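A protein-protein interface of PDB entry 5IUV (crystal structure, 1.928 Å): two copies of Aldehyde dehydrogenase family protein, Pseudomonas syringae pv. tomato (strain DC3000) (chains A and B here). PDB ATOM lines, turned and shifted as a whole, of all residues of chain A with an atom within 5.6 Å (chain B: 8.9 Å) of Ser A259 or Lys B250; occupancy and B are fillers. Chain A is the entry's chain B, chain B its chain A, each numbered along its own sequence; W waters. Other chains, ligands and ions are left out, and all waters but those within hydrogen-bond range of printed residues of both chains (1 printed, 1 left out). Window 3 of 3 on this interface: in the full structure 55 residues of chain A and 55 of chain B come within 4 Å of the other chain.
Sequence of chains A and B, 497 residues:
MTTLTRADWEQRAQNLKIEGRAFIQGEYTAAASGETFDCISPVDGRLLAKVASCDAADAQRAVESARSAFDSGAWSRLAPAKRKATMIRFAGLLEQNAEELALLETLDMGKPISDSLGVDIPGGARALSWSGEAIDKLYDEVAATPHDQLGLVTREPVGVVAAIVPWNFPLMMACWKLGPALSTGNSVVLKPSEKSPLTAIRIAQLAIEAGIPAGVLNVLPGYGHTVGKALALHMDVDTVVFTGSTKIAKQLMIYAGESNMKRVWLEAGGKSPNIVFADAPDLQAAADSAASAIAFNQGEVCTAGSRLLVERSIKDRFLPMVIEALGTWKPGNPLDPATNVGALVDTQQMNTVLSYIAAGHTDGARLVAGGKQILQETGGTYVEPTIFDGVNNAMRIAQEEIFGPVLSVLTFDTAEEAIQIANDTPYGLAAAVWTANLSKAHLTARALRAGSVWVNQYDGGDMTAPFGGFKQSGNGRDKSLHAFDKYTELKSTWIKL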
ATOM      1  N   ALA A 232      -6.109   8.211  20.509  1.00  0.00           N
ATOM      2  CA  ALA A 232      -5.133   9.140  19.956  1.00  0.00           C
ATOM      3  C   ALA A 232      -3.902   9.252  20.847  1.00  0.00           C
ATOM      4  O   ALA A 232      -2.810   9.537  20.363  1.00  0.00           O
ATOM      5  CB  ALA A 232      -5.771  10.508  19.741  1.00  0.00           C
ATOM      6  N   LEU A 233      -4.081   9.006  22.144  1.00  0.00           N
ATOM      7  CA  LEU A 233      -2.975   9.045  23.101  1.00  0.00           C
ATOM      8  C   LEU A 233      -2.352   7.672  23.348  1.00  0.00           C
ATOM      9  O   LEU A 233      -1.418   7.552  24.138  1.00  0.00           O
ATOM     10  CB  LEU A 233      -3.445   9.629  24.444  1.00  0.00           C
ATOM     11  CG  LEU A 233      -3.662  11.141  24.523  1.00  0.00           C
ATOM     12  CD1 LEU A 233      -4.382  11.512  25.824  1.00  0.00           C
ATOM     13  CD2 LEU A 233      -2.334  11.874  24.416  1.00  0.00           C
ATOM     14  N   HIS A 234      -2.863   6.632  22.695  1.00  0.00           N
ATOM     15  CA  HIS A 234      -2.429   5.288  23.062  1.00  0.00           C
ATOM     16  C   HIS A 234      -1.020   5.012  22.564  1.00  0.00           C
ATOM     17  O   HIS A 234      -0.686   5.306  21.419  1.00  0.00           O
ATOM     18  CB  HIS A 234      -3.387   4.220  22.545  1.00  0.00           C
ATOM     19  CG  HIS A 234      -3.296   2.937  23.309  1.00  0.00           C
ATOM     20  ND1 HIS A 234      -2.278   2.029  23.120  1.00  0.00           N
ATOM     21  CD2 HIS A 234      -4.086   2.425  24.283  1.00  0.00           C
ATOM     22  CE1 HIS A 234      -2.447   1.007  23.944  1.00  0.00           C
ATOM     23  NE2 HIS A 234      -3.538   1.221  24.655  1.00  0.00           N
ATOM     24  N   MET A 235      -0.204   4.439  23.441  1.00  0.00           N
ATOM     25  CA  MET A 235       1.207   4.227  23.152  1.00  0.00           C
ATOM     26  C   MET A 235       1.474   3.045  22.220  1.00  0.00           C
ATOM     27  O   MET A 235       2.609   2.855  21.780  1.00  0.00           O
ATOM     28  CB  MET A 235       1.979   4.042  24.460  1.00  0.00           C
ATOM     29  CG  MET A 235       1.971   5.269  25.354  1.00  0.00           C
ATOM     30  SD  MET A 235       2.831   6.679  24.621  1.00  0.00           S
ATOM     31  CE  MET A 235       4.530   6.111  24.648  1.00  0.00           C
ATOM     32  N   ILE A 254      -1.368  17.207  18.609  1.00  0.00           N
ATOM     33  CA  ILE A 254      -0.879  17.412  19.963  1.00  0.00           C
ATOM     34  C   ILE A 254      -0.865  16.081  20.724  1.00  0.00           C
ATOM     35  O   ILE A 254       0.129  15.754  21.372  1.00  0.00           O
ATOM     36  CB  ILE A 254      -1.733  18.467  20.705  1.00  0.00           C
ATOM     37  CG1 ILE A 254      -1.532  19.845  20.070  1.00  0.00           C
ATOM     38  CG2 ILE A 254      -1.388  18.519  22.193  1.00  0.00           C
ATOM     39  CD1 ILE A 254      -2.394  20.948  20.695  1.00  0.00           C
ATOM     40  N   TYR A 255      -1.941  15.296  20.617  1.00  0.00           N
ATOM     41  CA  TYR A 255      -1.979  13.988  21.272  1.00  0.00           C
ATOM     42  C   TYR A 255      -0.834  13.081  20.820  1.00  0.00           C
ATOM     43  O   TYR A 255      -0.230  12.387  21.641  1.00  0.00           O
ATOM     44  CB  TYR A 255      -3.309  13.269  21.014  1.00  0.00           C
ATOM     45  CG  TYR A 255      -4.524  13.900  21.658  1.00  0.00           C
ATOM     46  CD1 TYR A 255      -4.424  14.618  22.847  1.00  0.00           C
ATOM     47  CD2 TYR A 255      -5.777  13.770  21.075  1.00  0.00           C
ATOM     48  CE1 TYR A 255      -5.547  15.193  23.433  1.00  0.00           C
ATOM     49  CE2 TYR A 255      -6.902  14.333  21.649  1.00  0.00           C
ATOM     50  CZ  TYR A 255      -6.786  15.041  22.827  1.00  0.00           C
ATOM     51  OH  TYR A 255      -7.914  15.600  23.383  1.00  0.00           O
ATOM     52  N   ALA A 256      -0.549  13.066  19.520  1.00  0.00           N
ATOM     53  CA  ALA A 256       0.531  12.233  18.999  1.00  0.00           C
ATOM     54  C   ALA A 256       1.878  12.652  19.574  1.00  0.00           C
ATOM     55  O   ALA A 256       2.687  11.807  19.959  1.00  0.00           O
ATOM     56  CB  ALA A 256       0.568  12.298  17.487  1.00  0.00           C
ATOM     57  N   GLY A 257       2.110  13.957  19.630  1.00  0.00           N
ATOM     58  CA  GLY A 257       3.329  14.496  20.207  1.00  0.00           C
ATOM     59  C   GLY A 257       3.459  14.237  21.697  1.00  0.00           C
ATOM     60  O   GLY A 257       4.566  14.065  22.206  1.00  0.00           O
ATOM     61  N   GLU A 258       2.329  14.207  22.397  1.00  0.00           N
ATOM     62  CA  GLU A 258       2.325  13.941  23.831  1.00  0.00           C
ATOM     63  C   GLU A 258       2.543  12.470  24.149  1.00  0.00           C
ATOM     64  O   GLU A 258       2.890  12.134  25.273  1.00  0.00           O
ATOM     65  CB  GLU A 258       1.003  14.391  24.466  1.00  0.00           C
ATOM     66  CG  GLU A 258       0.820  15.896  24.552  1.00  0.00           C
ATOM     67  CD  GLU A 258      -0.524  16.271  25.139  1.00  0.00           C
ATOM     68  OE1 GLU A 258      -1.403  15.386  25.214  1.00  0.00           O
ATOM     69  OE2 GLU A 258      -0.706  17.441  25.528  1.00  0.00           O
ATOM     70  N   SER A 259       2.313  11.598  23.170  1.00  0.00           N
ATOM     71  CA  SER A 259       2.358  10.161  23.418  1.00  0.00           C
ATOM     72  C   SER A 259       3.526   9.481  22.701  1.00  0.00           C
ATOM     73  O   SER A 259       4.659   9.545  23.176  1.00  0.00           O
ATOM     74  CB  SER A 259       1.023   9.505  23.019  1.00  0.00           C
ATOM     75  OG  SER A 259       0.711   9.722  21.654  1.00  0.00           O
ATOM     76  N   ASN A 260       3.262   8.839  21.564  1.00  0.00           N
ATOM     77  CA  ASN A 260       4.263   7.971  20.940  1.00  0.00           C
ATOM     78  C   ASN A 260       4.684   8.368  19.523  1.00  0.00           C
ATOM     79  O   ASN A 260       5.212   7.538  18.785  1.00  0.00           O
ATOM     80  CB  ASN A 260       3.742   6.526  20.908  1.00  0.00           C
ATOM     81  CG  ASN A 260       2.592   6.340  19.919  1.00  0.00           C
ATOM     82  OD1 ASN A 260       1.945   7.304  19.506  1.00  0.00           O
ATOM     83  ND2 ASN A 260       2.335   5.097  19.544  1.00  0.00           N
ATOM     84  N   MET A 261       4.443   9.622  19.146  1.00  0.00           N
ATOM     85  CA  MET A 261       4.786  10.108  17.815  1.00  0.00           C
ATOM     86  C   MET A 261       4.104   9.292  16.717  1.00  0.00           C
ATOM     87  O   MET A 261       4.675   9.104  15.644  1.00  0.00           O
ATOM     88  CB  MET A 261       6.305  10.076  17.607  1.00  0.00           C
ATOM     89  CG  MET A 261       6.911  11.369  17.123  1.00  0.00           C
ATOM     90  SD  MET A 261       8.712  11.233  17.050  1.00  0.00           S
ATOM     91  CE  MET A 261       8.849  10.192  15.626  1.00  0.00           C
ATOM     92  N   LYS A 262       2.897   8.799  16.986  1.00  0.00           N
ATOM     93  CA  LYS A 262       2.147   8.053  15.975  1.00  0.00           C
ATOM     94  C   LYS A 262       1.939   8.915  14.732  1.00  0.00           C
ATOM     95  O   LYS A 262       1.911  10.140  14.821  1.00  0.00           O
ATOM     96  CB  LYS A 262       0.793   7.582  16.531  1.00  0.00           C
ATOM     97  CG  LYS A 262      -0.076   8.694  17.126  1.00  0.00           C
ATOM     98  CD  LYS A 262      -1.473   8.182  17.504  1.00  0.00           C
ATOM     99  CE  LYS A 262      -1.417   7.077  18.557  1.00  0.00           C
ATOM    100  NZ  LYS A 262      -0.925   7.544  19.890  1.00  0.00           N
ATOM    101  N   PHE B 242      12.436  17.908   9.937  1.00  0.00           N
ATOM    102  CA  PHE B 242      13.274  17.896  11.121  1.00  0.00           C
ATOM    103  C   PHE B 242      14.146  16.662  11.167  1.00  0.00           C
ATOM    104  O   PHE B 242      13.704  15.564  10.844  1.00  0.00           O
ATOM    105  CB  PHE B 242      12.393  17.958  12.375  1.00  0.00           C
ATOM    106  CG  PHE B 242      13.141  17.773  13.678  1.00  0.00           C
ATOM    107  CD1 PHE B 242      13.196  16.530  14.293  1.00  0.00           C
ATOM    108  CD2 PHE B 242      13.754  18.850  14.302  1.00  0.00           C
ATOM    109  CE1 PHE B 242      13.870  16.357  15.495  1.00  0.00           C
ATOM    110  CE2 PHE B 242      14.429  18.686  15.500  1.00  0.00           C
ATOM    111  CZ  PHE B 242      14.484  17.437  16.100  1.00  0.00           C
ATOM    112  N   GLY B 244      16.738  15.178  14.250  1.00  0.00           N
ATOM    113  CA  GLY B 244      17.229  15.418  15.590  1.00  0.00           C
ATOM    114  C   GLY B 244      16.747  14.361  16.561  1.00  0.00           C
ATOM    115  O   GLY B 244      16.487  13.224  16.169  1.00  0.00           O
ATOM    116  N   SER B 245      16.647  14.731  17.832  1.00  0.00           N
ATOM    117  CA  SER B 245      16.224  13.805  18.865  1.00  0.00           C
ATOM    118  C   SER B 245      14.729  13.515  18.785  1.00  0.00           C
ATOM    119  O   SER B 245      13.945  14.301  18.246  1.00  0.00           O
ATOM    120  CB  SER B 245      16.573  14.345  20.258  1.00  0.00           C
ATOM    121  OG  SER B 245      15.776  15.466  20.608  1.00  0.00           O
ATOM    122  N   THR B 246      14.346  12.369  19.328  1.00  0.00           N
ATOM    123  CA  THR B 246      12.948  11.983  19.389  1.00  0.00           C
ATOM    124  C   THR B 246      12.161  12.947  20.271  1.00  0.00           C
ATOM    125  O   THR B 246      11.026  13.292  19.961  1.00  0.00           O
ATOM    126  CB  THR B 246      12.799  10.542  19.910  1.00  0.00           C
ATOM    127  OG1 THR B 246      13.344   9.634  18.940  1.00  0.00           O
ATOM    128  CG2 THR B 246      11.330  10.202  20.143  1.00  0.00           C
ATOM    129  N   LYS B 247      12.772  13.394  21.361  1.00  0.00           N
ATOM    130  CA  LYS B 247      12.111  14.321  22.277  1.00  0.00           C
ATOM    131  C   LYS B 247      11.666  15.628  21.608  1.00  0.00           C
ATOM    132  O   LYS B 247      10.530  16.079  21.794  1.00  0.00           O
ATOM    133  CB  LYS B 247      13.028  14.642  23.453  1.00  0.00           C
ATOM    134  CG  LYS B 247      12.437  15.634  24.435  1.00  0.00           C
ATOM    135  CD  LYS B 247      13.510  16.206  25.348  1.00  0.00           C
ATOM    136  CE  LYS B 247      12.912  17.110  26.411  1.00  0.00           C
ATOM    137  NZ  LYS B 247      12.063  16.335  27.354  1.00  0.00           N
ATOM    138  N   ILE B 248      12.565  16.243  20.848  1.00  0.00           N
ATOM    139  CA  ILE B 248      12.239  17.482  20.150  1.00  0.00           C
ATOM    140  C   ILE B 248      11.302  17.209  18.974  1.00  0.00           C
ATOM    141  O   ILE B 248      10.419  18.009  18.675  1.00  0.00           O
ATOM    142  CB  ILE B 248      13.508  18.202  19.643  1.00  0.00           C
ATOM    143  CG1 ILE B 248      14.407  18.584  20.822  1.00  0.00           C
ATOM    144  CG2 ILE B 248      13.139  19.452  18.843  1.00  0.00           C
ATOM    145  CD1 ILE B 248      13.735  19.506  21.820  1.00  0.00           C
ATOM    146  N   ALA B 249      11.492  16.071  18.319  1.00  0.00           N
ATOM    147  CA  ALA B 249      10.620  15.680  17.217  1.00  0.00           C
ATOM    148  C   ALA B 249       9.156  15.655  17.652  1.00  0.00           C
ATOM    149  O   ALA B 249       8.295  16.193  16.959  1.00  0.00           O
ATOM    150  CB  ALA B 249      11.041  14.315  16.658  1.00  0.00           C
ATOM    151  N   LYS B 250       8.881  15.055  18.808  1.00  0.00           N
ATOM    152  CA  LYS B 250       7.531  15.038  19.363  1.00  0.00           C
ATOM    153  C   LYS B 250       6.986  16.439  19.626  1.00  0.00           C
ATOM    154  O   LYS B 250       5.811  16.705  19.382  1.00  0.00           O
ATOM    155  CB  LYS B 250       7.490  14.216  20.661  1.00  0.00           C
ATOM    156  CG  LYS B 250       7.560  12.711  20.469  1.00  0.00           C
ATOM    157  CD  LYS B 250       7.762  12.042  21.814  1.00  0.00           C
ATOM    158  CE  LYS B 250       7.690  10.547  21.694  1.00  0.00           C
ATOM    159  NZ  LYS B 250       7.956   9.878  23.002  1.00  0.00           N
ATOM    160  N   GLN B 251       7.839  17.328  20.125  1.00  0.00           N
ATOM    161  CA  GLN B 251       7.434  18.691  20.426  1.00  0.00           C
ATOM    162  C   GLN B 251       7.014  19.442  19.164  1.00  0.00           C
ATOM    163  O   GLN B 251       6.177  20.334  19.225  1.00  0.00           O
ATOM    164  CB  GLN B 251       8.572  19.433  21.132  1.00  0.00           C
ATOM    165  CG  GLN B 251       8.194  20.825  21.660  1.00  0.00           C
ATOM    166  CD  GLN B 251       7.079  20.840  22.705  1.00  0.00           C
ATOM    167  OE1 GLN B 251       6.059  21.505  22.525  1.00  0.00           O
ATOM    168  NE2 GLN B 251       7.292  20.148  23.817  1.00  0.00           N
ATOM    169  N   LEU B 252       7.596  19.085  18.022  1.00  0.00           N
ATOM    170  CA  LEU B 252       7.220  19.730  16.759  1.00  0.00           C
ATOM    171  C   LEU B 252       5.787  19.361  16.358  1.00  0.00           C
ATOM    172  O   LEU B 252       5.070  20.173  15.782  1.00  0.00           O
ATOM    173  CB  LEU B 252       8.188  19.356  15.623  1.00  0.00           C
ATOM    174  CG  LEU B 252       9.677  19.728  15.722  1.00  0.00           C
ATOM    175  CD1 LEU B 252      10.275  19.822  14.328  1.00  0.00           C
ATOM    176  CD2 LEU B 252       9.914  21.019  16.502  1.00  0.00           C
ATOM    177  N   MET B 253       5.374  18.137  16.651  1.00  0.00           N
ATOM    178  CA  MET B 253       3.992  17.739  16.384  1.00  0.00           C
ATOM    179  C   MET B 253       3.034  18.576  17.224  1.00  0.00           C
ATOM    180  O   MET B 253       1.970  18.992  16.763  1.00  0.00           O
ATOM    181  CB  MET B 253       3.797  16.255  16.669  1.00  0.00           C
ATOM    182  CG  MET B 253       4.635  15.353  15.796  1.00  0.00           C
ATOM    183  SD  MET B 253       4.087  13.641  15.848  1.00  0.00           S
ATOM    184  CE  MET B 253       2.590  13.719  14.856  1.00  0.00           C
ATOM    185  N   ILE B 254       3.439  18.841  18.460  1.00  0.00           N
ATOM    186  CA  ILE B 254       2.652  19.676  19.350  1.00  0.00           C
ATOM    187  C   ILE B 254       2.592  21.120  18.829  1.00  0.00           C
ATOM    188  O   ILE B 254       1.511  21.718  18.783  1.00  0.00           O
ATOM    189  CB  ILE B 254       3.214  19.638  20.785  1.00  0.00           C
ATOM    190  CG1 ILE B 254       3.073  18.220  21.351  1.00  0.00           C
ATOM    191  CG2 ILE B 254       2.517  20.674  21.662  1.00  0.00           C
ATOM    192  CD1 ILE B 254       3.682  18.018  22.717  1.00  0.00           C
ATOM    193  N   TYR B 255       3.734  21.662  18.408  1.00  0.00           N
ATOM    194  CA  TYR B 255       3.771  23.011  17.836  1.00  0.00           C
ATOM    195  C   TYR B 255       2.867  23.153  16.613  1.00  0.00           C
ATOM    196  O   TYR B 255       2.210  24.175  16.436  1.00  0.00           O
ATOM    197  CB  TYR B 255       5.190  23.408  17.427  1.00  0.00           C
ATOM    198  CG  TYR B 255       6.189  23.569  18.550  1.00  0.00           C
ATOM    199  CD1 TYR B 255       5.801  23.983  19.817  1.00  0.00           C
ATOM    200  CD2 TYR B 255       7.538  23.316  18.330  1.00  0.00           C
ATOM    201  CE1 TYR B 255       6.738  24.134  20.839  1.00  0.00           C
ATOM    202  CE2 TYR B 255       8.475  23.464  19.333  1.00  0.00           C
ATOM    203  CZ  TYR B 255       8.073  23.874  20.586  1.00  0.00           C
ATOM    204  OH  TYR B 255       9.023  24.015  21.581  1.00  0.00           O
ATOM    205  N   ALA B 256       2.855  22.143  15.751  1.00  0.00           N
ATOM    206  CA  ALA B 256       2.008  22.198  14.567  1.00  0.00           C
ATOM    207  C   ALA B 256       0.538  22.233  14.968  1.00  0.00           C
ATOM    208  O   ALA B 256      -0.254  22.992  14.401  1.00  0.00           O
ATOM    209  CB  ALA B 256       2.284  21.023  13.669  1.00  0.00           C
ATOM    210  N   GLY B 257       0.182  21.409  15.950  1.00  0.00           N
ATOM    211  CA  GLY B 257      -1.174  21.369  16.470  1.00  0.00           C
ATOM    212  C   GLY B 257      -1.604  22.669  17.135  1.00  0.00           C
ATOM    213  O   GLY B 257      -2.771  23.053  17.077  1.00  0.00           O
ATOM    214  N   VAL B 264       4.298  17.894   9.244  1.00  0.00           N
ATOM    215  CA  VAL B 264       5.467  17.631  10.075  1.00  0.00           C
ATOM    216  C   VAL B 264       6.117  16.322   9.651  1.00  0.00           C
ATOM    217  O   VAL B 264       5.471  15.278   9.659  1.00  0.00           O
ATOM    218  CB  VAL B 264       5.093  17.551  11.575  1.00  0.00           C
ATOM    219  CG1 VAL B 264       6.305  17.184  12.423  1.00  0.00           C
ATOM    220  CG2 VAL B 264       4.497  18.859  12.045  1.00  0.00           C
ATOM    221  N   LEU B 266       9.531  13.905  10.335  1.00  0.00           N
ATOM    222  CA  LEU B 266      10.544  13.729  11.370  1.00  0.00           C
ATOM    223  C   LEU B 266      11.534  12.615  11.061  1.00  0.00           C
ATOM    224  O   LEU B 266      11.149  11.530  10.625  1.00  0.00           O
ATOM    225  CB  LEU B 266       9.868  13.431  12.716  1.00  0.00           C
ATOM    226  CG  LEU B 266       8.748  14.396  13.114  1.00  0.00           C
ATOM    227  CD1 LEU B 266       7.888  13.830  14.243  1.00  0.00           C
ATOM    228  CD2 LEU B 266       9.351  15.735  13.500  1.00  0.00           C
ATOM    229  N   GLU B 267      12.808  12.893  11.312  1.00  0.00           N
ATOM    230  CA  GLU B 267      13.852  11.879  11.304  1.00  0.00           C
ATOM    231  C   GLU B 267      14.522  11.944  12.669  1.00  0.00           C
ATOM    232  O   GLU B 267      15.193  12.921  12.977  1.00  0.00           O
ATOM    233  CB  GLU B 267      14.862  12.127  10.182  1.00  0.00           C
ATOM    234  CG  GLU B 267      14.260  12.141   8.781  1.00  0.00           C
ATOM    235  CD  GLU B 267      14.526  10.848   8.023  1.00  0.00           C
ATOM    236  OE1 GLU B 267      15.322  10.023   8.526  1.00  0.00           O
ATOM    237  OE2 GLU B 267      13.952  10.663   6.928  1.00  0.00           O
ATOM    238  N   ALA B 268      14.329  10.922  13.494  1.00  0.00           N
ATOM    239  CA  ALA B 268      14.704  11.025  14.894  1.00  0.00           C
ATOM    240  C   ALA B 268      15.733   9.975  15.290  1.00  0.00           C
ATOM    241  O   ALA B 268      16.507   9.510  14.461  1.00  0.00           O
ATOM    242  CB  ALA B 268      13.471  10.924  15.778  1.00  0.00           C
ATOM    243  N   PRO B 426      11.575   1.273  21.158  1.00  0.00           N
ATOM    244  CA  PRO B 426      10.631   2.262  20.628  1.00  0.00           C
ATOM    245  C   PRO B 426      11.094   2.810  19.290  1.00  0.00           C
ATOM    246  O   PRO B 426      10.347   3.520  18.619  1.00  0.00           O
ATOM    247  CB  PRO B 426      10.642   3.366  21.690  1.00  0.00           C
ATOM    248  CG  PRO B 426      11.998   3.278  22.279  1.00  0.00           C
ATOM    249  CD  PRO B 426      12.344   1.810  22.296  1.00  0.00           C
ATOM    250  N   TYR B 427      12.329   2.489  18.921  1.00  0.00           N
ATOM    251  CA  TYR B 427      12.931   3.010  17.700  1.00  0.00           C
ATOM    252  C   TYR B 427      12.733   2.067  16.511  1.00  0.00           C
ATOM    253  O   TYR B 427      12.141   1.000  16.651  1.00  0.00           O
ATOM    254  CB  TYR B 427      14.419   3.259  17.923  1.00  0.00           C
ATOM    255  CG  TYR B 427      14.714   4.366  18.910  1.00  0.00           C
ATOM    256  CD1 TYR B 427      14.358   5.682  18.631  1.00  0.00           C
ATOM    257  CD2 TYR B 427      15.367   4.103  20.106  1.00  0.00           C
ATOM    258  CE1 TYR B 427      14.640   6.708  19.524  1.00  0.00           C
ATOM    259  CE2 TYR B 427      15.651   5.123  21.011  1.00  0.00           C
ATOM    260  CZ  TYR B 427      15.287   6.423  20.709  1.00  0.00           C
ATOM    261  OH  TYR B 427      15.566   7.444  21.589  1.00  0.00           O
ATOM    262  N   LYS B 471       8.076   3.762  13.718  1.00  0.00           N
ATOM    263  CA  LYS B 471       7.802   4.096  15.119  1.00  0.00           C
ATOM    264  C   LYS B 471       8.424   5.428  15.544  1.00  0.00           C
ATOM    265  O   LYS B 471       8.290   6.419  14.835  1.00  0.00           O
ATOM    266  CB  LYS B 471       8.282   2.957  16.026  1.00  0.00           C
ATOM    267  CG  LYS B 471       7.549   1.635  15.778  1.00  0.00           C
ATOM    268  CD  LYS B 471       7.934   0.560  16.788  1.00  0.00           C
ATOM    269  CE  LYS B 471       9.157  -0.215  16.338  1.00  0.00           C
ATOM    270  NZ  LYS B 471       9.471  -1.357  17.261  1.00  0.00           N
ATOM    271  N   GLN B 472       9.115   5.452  16.682  1.00  0.00           N
ATOM    272  CA  GLN B 472       9.571   6.730  17.218  1.00  0.00           C
ATOM    273  C   GLN B 472      10.898   7.201  16.610  1.00  0.00           C
ATOM    274  O   GLN B 472      11.501   8.146  17.099  1.00  0.00           O
ATOM    275  CB  GLN B 472       9.670   6.658  18.751  1.00  0.00           C
ATOM    276  CG  GLN B 472       8.328   6.364  19.426  1.00  0.00           C
ATOM    277  CD  GLN B 472       8.320   6.715  20.903  1.00  0.00           C
ATOM    278  OE1 GLN B 472       8.847   7.745  21.310  1.00  0.00           O
ATOM    279  NE2 GLN B 472       7.723   5.850  21.711  1.00  0.00           N
ATOM    280  N   SER B 473      11.331   6.550  15.534  1.00  0.00           N
ATOM    281  CA  SER B 473      12.488   7.019  14.775  1.00  0.00           C
ATOM    282  C   SER B 473      12.069   8.009  13.684  1.00  0.00           C
ATOM    283  O   SER B 473      12.909   8.548  12.964  1.00  0.00           O
ATOM    284  CB  SER B 473      13.247   5.839  14.157  1.00  0.00           C
ATOM    285  OG  SER B 473      13.956   5.120  15.158  1.00  0.00           O
ATOM    286  N   GLY B 474      10.769   8.238  13.552  1.00  0.00           N
ATOM    287  CA  GLY B 474      10.292   9.272  12.652  1.00  0.00           C
ATOM    288  C   GLY B 474       9.220   8.862  11.661  1.00  0.00           C
ATOM    289  O   GLY B 474       8.702   7.746  11.702  1.00  0.00           O
ATOM    290  N   ASN B 475       8.885   9.788  10.768  1.00  0.00           N
ATOM    291  CA  ASN B 475       7.938   9.515   9.692  1.00  0.00           C
ATOM    292  C   ASN B 475       8.434  10.156   8.404  1.00  0.00           C
ATOM    293  O   ASN B 475       9.070  11.213   8.431  1.00  0.00           O
ATOM    294  CB  ASN B 475       6.537  10.038  10.038  1.00  0.00           C
ATOM    295  CG  ASN B 475       6.488  11.551  10.128  1.00  0.00           C
ATOM    296  OD1 ASN B 475       7.305  12.162  10.814  1.00  0.00           O
ATOM    297  ND2 ASN B 475       5.541  12.164   9.425  1.00  0.00           N
HETATM  298  O   HOH W   1       6.342  10.684  25.154  1.00  0.00           O
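Ile A254 touches its own counterpart, Ile B254. Ile A254 touches Gly B257, and with the chains exchanged Gly A257 touches Ile B254. Positions printed for both chains: 254, 255, 256 and 257. Of the 16 pairs that touch across the chains among the printed residues, 3 have their exchanged pair printed and touching as well.
Of the 26 printed residues of chain B, 9 touch a printed residue of chain A. Hydrophobic or aromatic side chains of chain B within 4 Å of the printed part of chain A: Ala B249, Met B253, Ile B254 and Leu B266. Of the 13 printed residues of chain A, 7 touch a printed residue of chain B. Hydrophobic or aromatic side chains of chain A within 4 Å of the printed part of chain B: Ile A254, Ala A256 and Met A261. Among the printed residues, no Asp or Glu carboxylate lies within 4 Å of a Lys or Arg side-chain nitrogen of the other chain.
Of chain B, only Lys B250 (3.3 Å), Met B253 (3.98 Å) and Ile B254 (3.9 Å) come within 4 Å of Gly A257. Of chain B, only Lys B250 (3.3 Å) comes within 4 Å of Ser A259. Printed residues of chain B within 4 Å of Asn A260: Gln B472. Of the printed residues of chain B, Lys A262 touches Met B253 (3.6 Å). Lys B250 touches just these residues of chain A: Gly A257, Ser A259 and Met A261. Of the printed residues of chain A, Met B253 touches Ala A256 (3.6 Å), Gly A257 (3.98 Å), Met A261 (3.8 Å) and Lys A262 (3.6 Å). The nearest residue of chain B that does not touch Ser A259 is Gln B472 (4.9 Å).
The backbone NH (N) of Asn B475 sits at hydrogen-bond distance from the backbone carbonyl oxygen (O) of Leu B266, 2.9 Å away. The backbone carbonyl oxygen (O) of Pro B426 is in hydrogen-bond range of the backbone NH (N) of Gln B472, at 3.0 Å. O of Ala A232 is in hydrogen-bond range of NZ of Lys A262, 2.8 Å away. The backbone carbonyl oxygen of Tyr A255 lies within hydrogen-bond range of the side-chain hydroxyl of Ser A259, 2.8 Å away. O of Ala A256 is in hydrogen-bond range of OG of Ser A259 (3.3 Å). The side-chain hydroxyl of Ser A259 sits at hydrogen-bond distance from the side-chain amino group of Lys A262 (3.2 Å).
Water W1 bridges the side-chain amino group (NZ) of Lys B250 and the backbone carbonyl oxygen (O) of Ser A259.
Ile A254 touches Ile B254. Ile A254 touches Gly B257 (CG1 to CA, 3.9 Å). Gly A257 touches Lys B250. Gly A257 touches Ile B254. Asn A260 touches Gln B472 (O to CG, 3.4 Å). Met A261 touches Lys B250. SD of Met B253 touches CG of Met A261, at 3.8 Å. Met A261 touches Lys B471 (CE to O, 3.9 Å). Gln B472 touches Met A261 (O to CE, 3.7 Å). O of Lys A262 touches CE of Met B253, 3.6 Å away.
The backbone carbonyl oxygen of Ser A259 sits at hydrogen-bond distance from the side-chain amino group of Lys B250.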
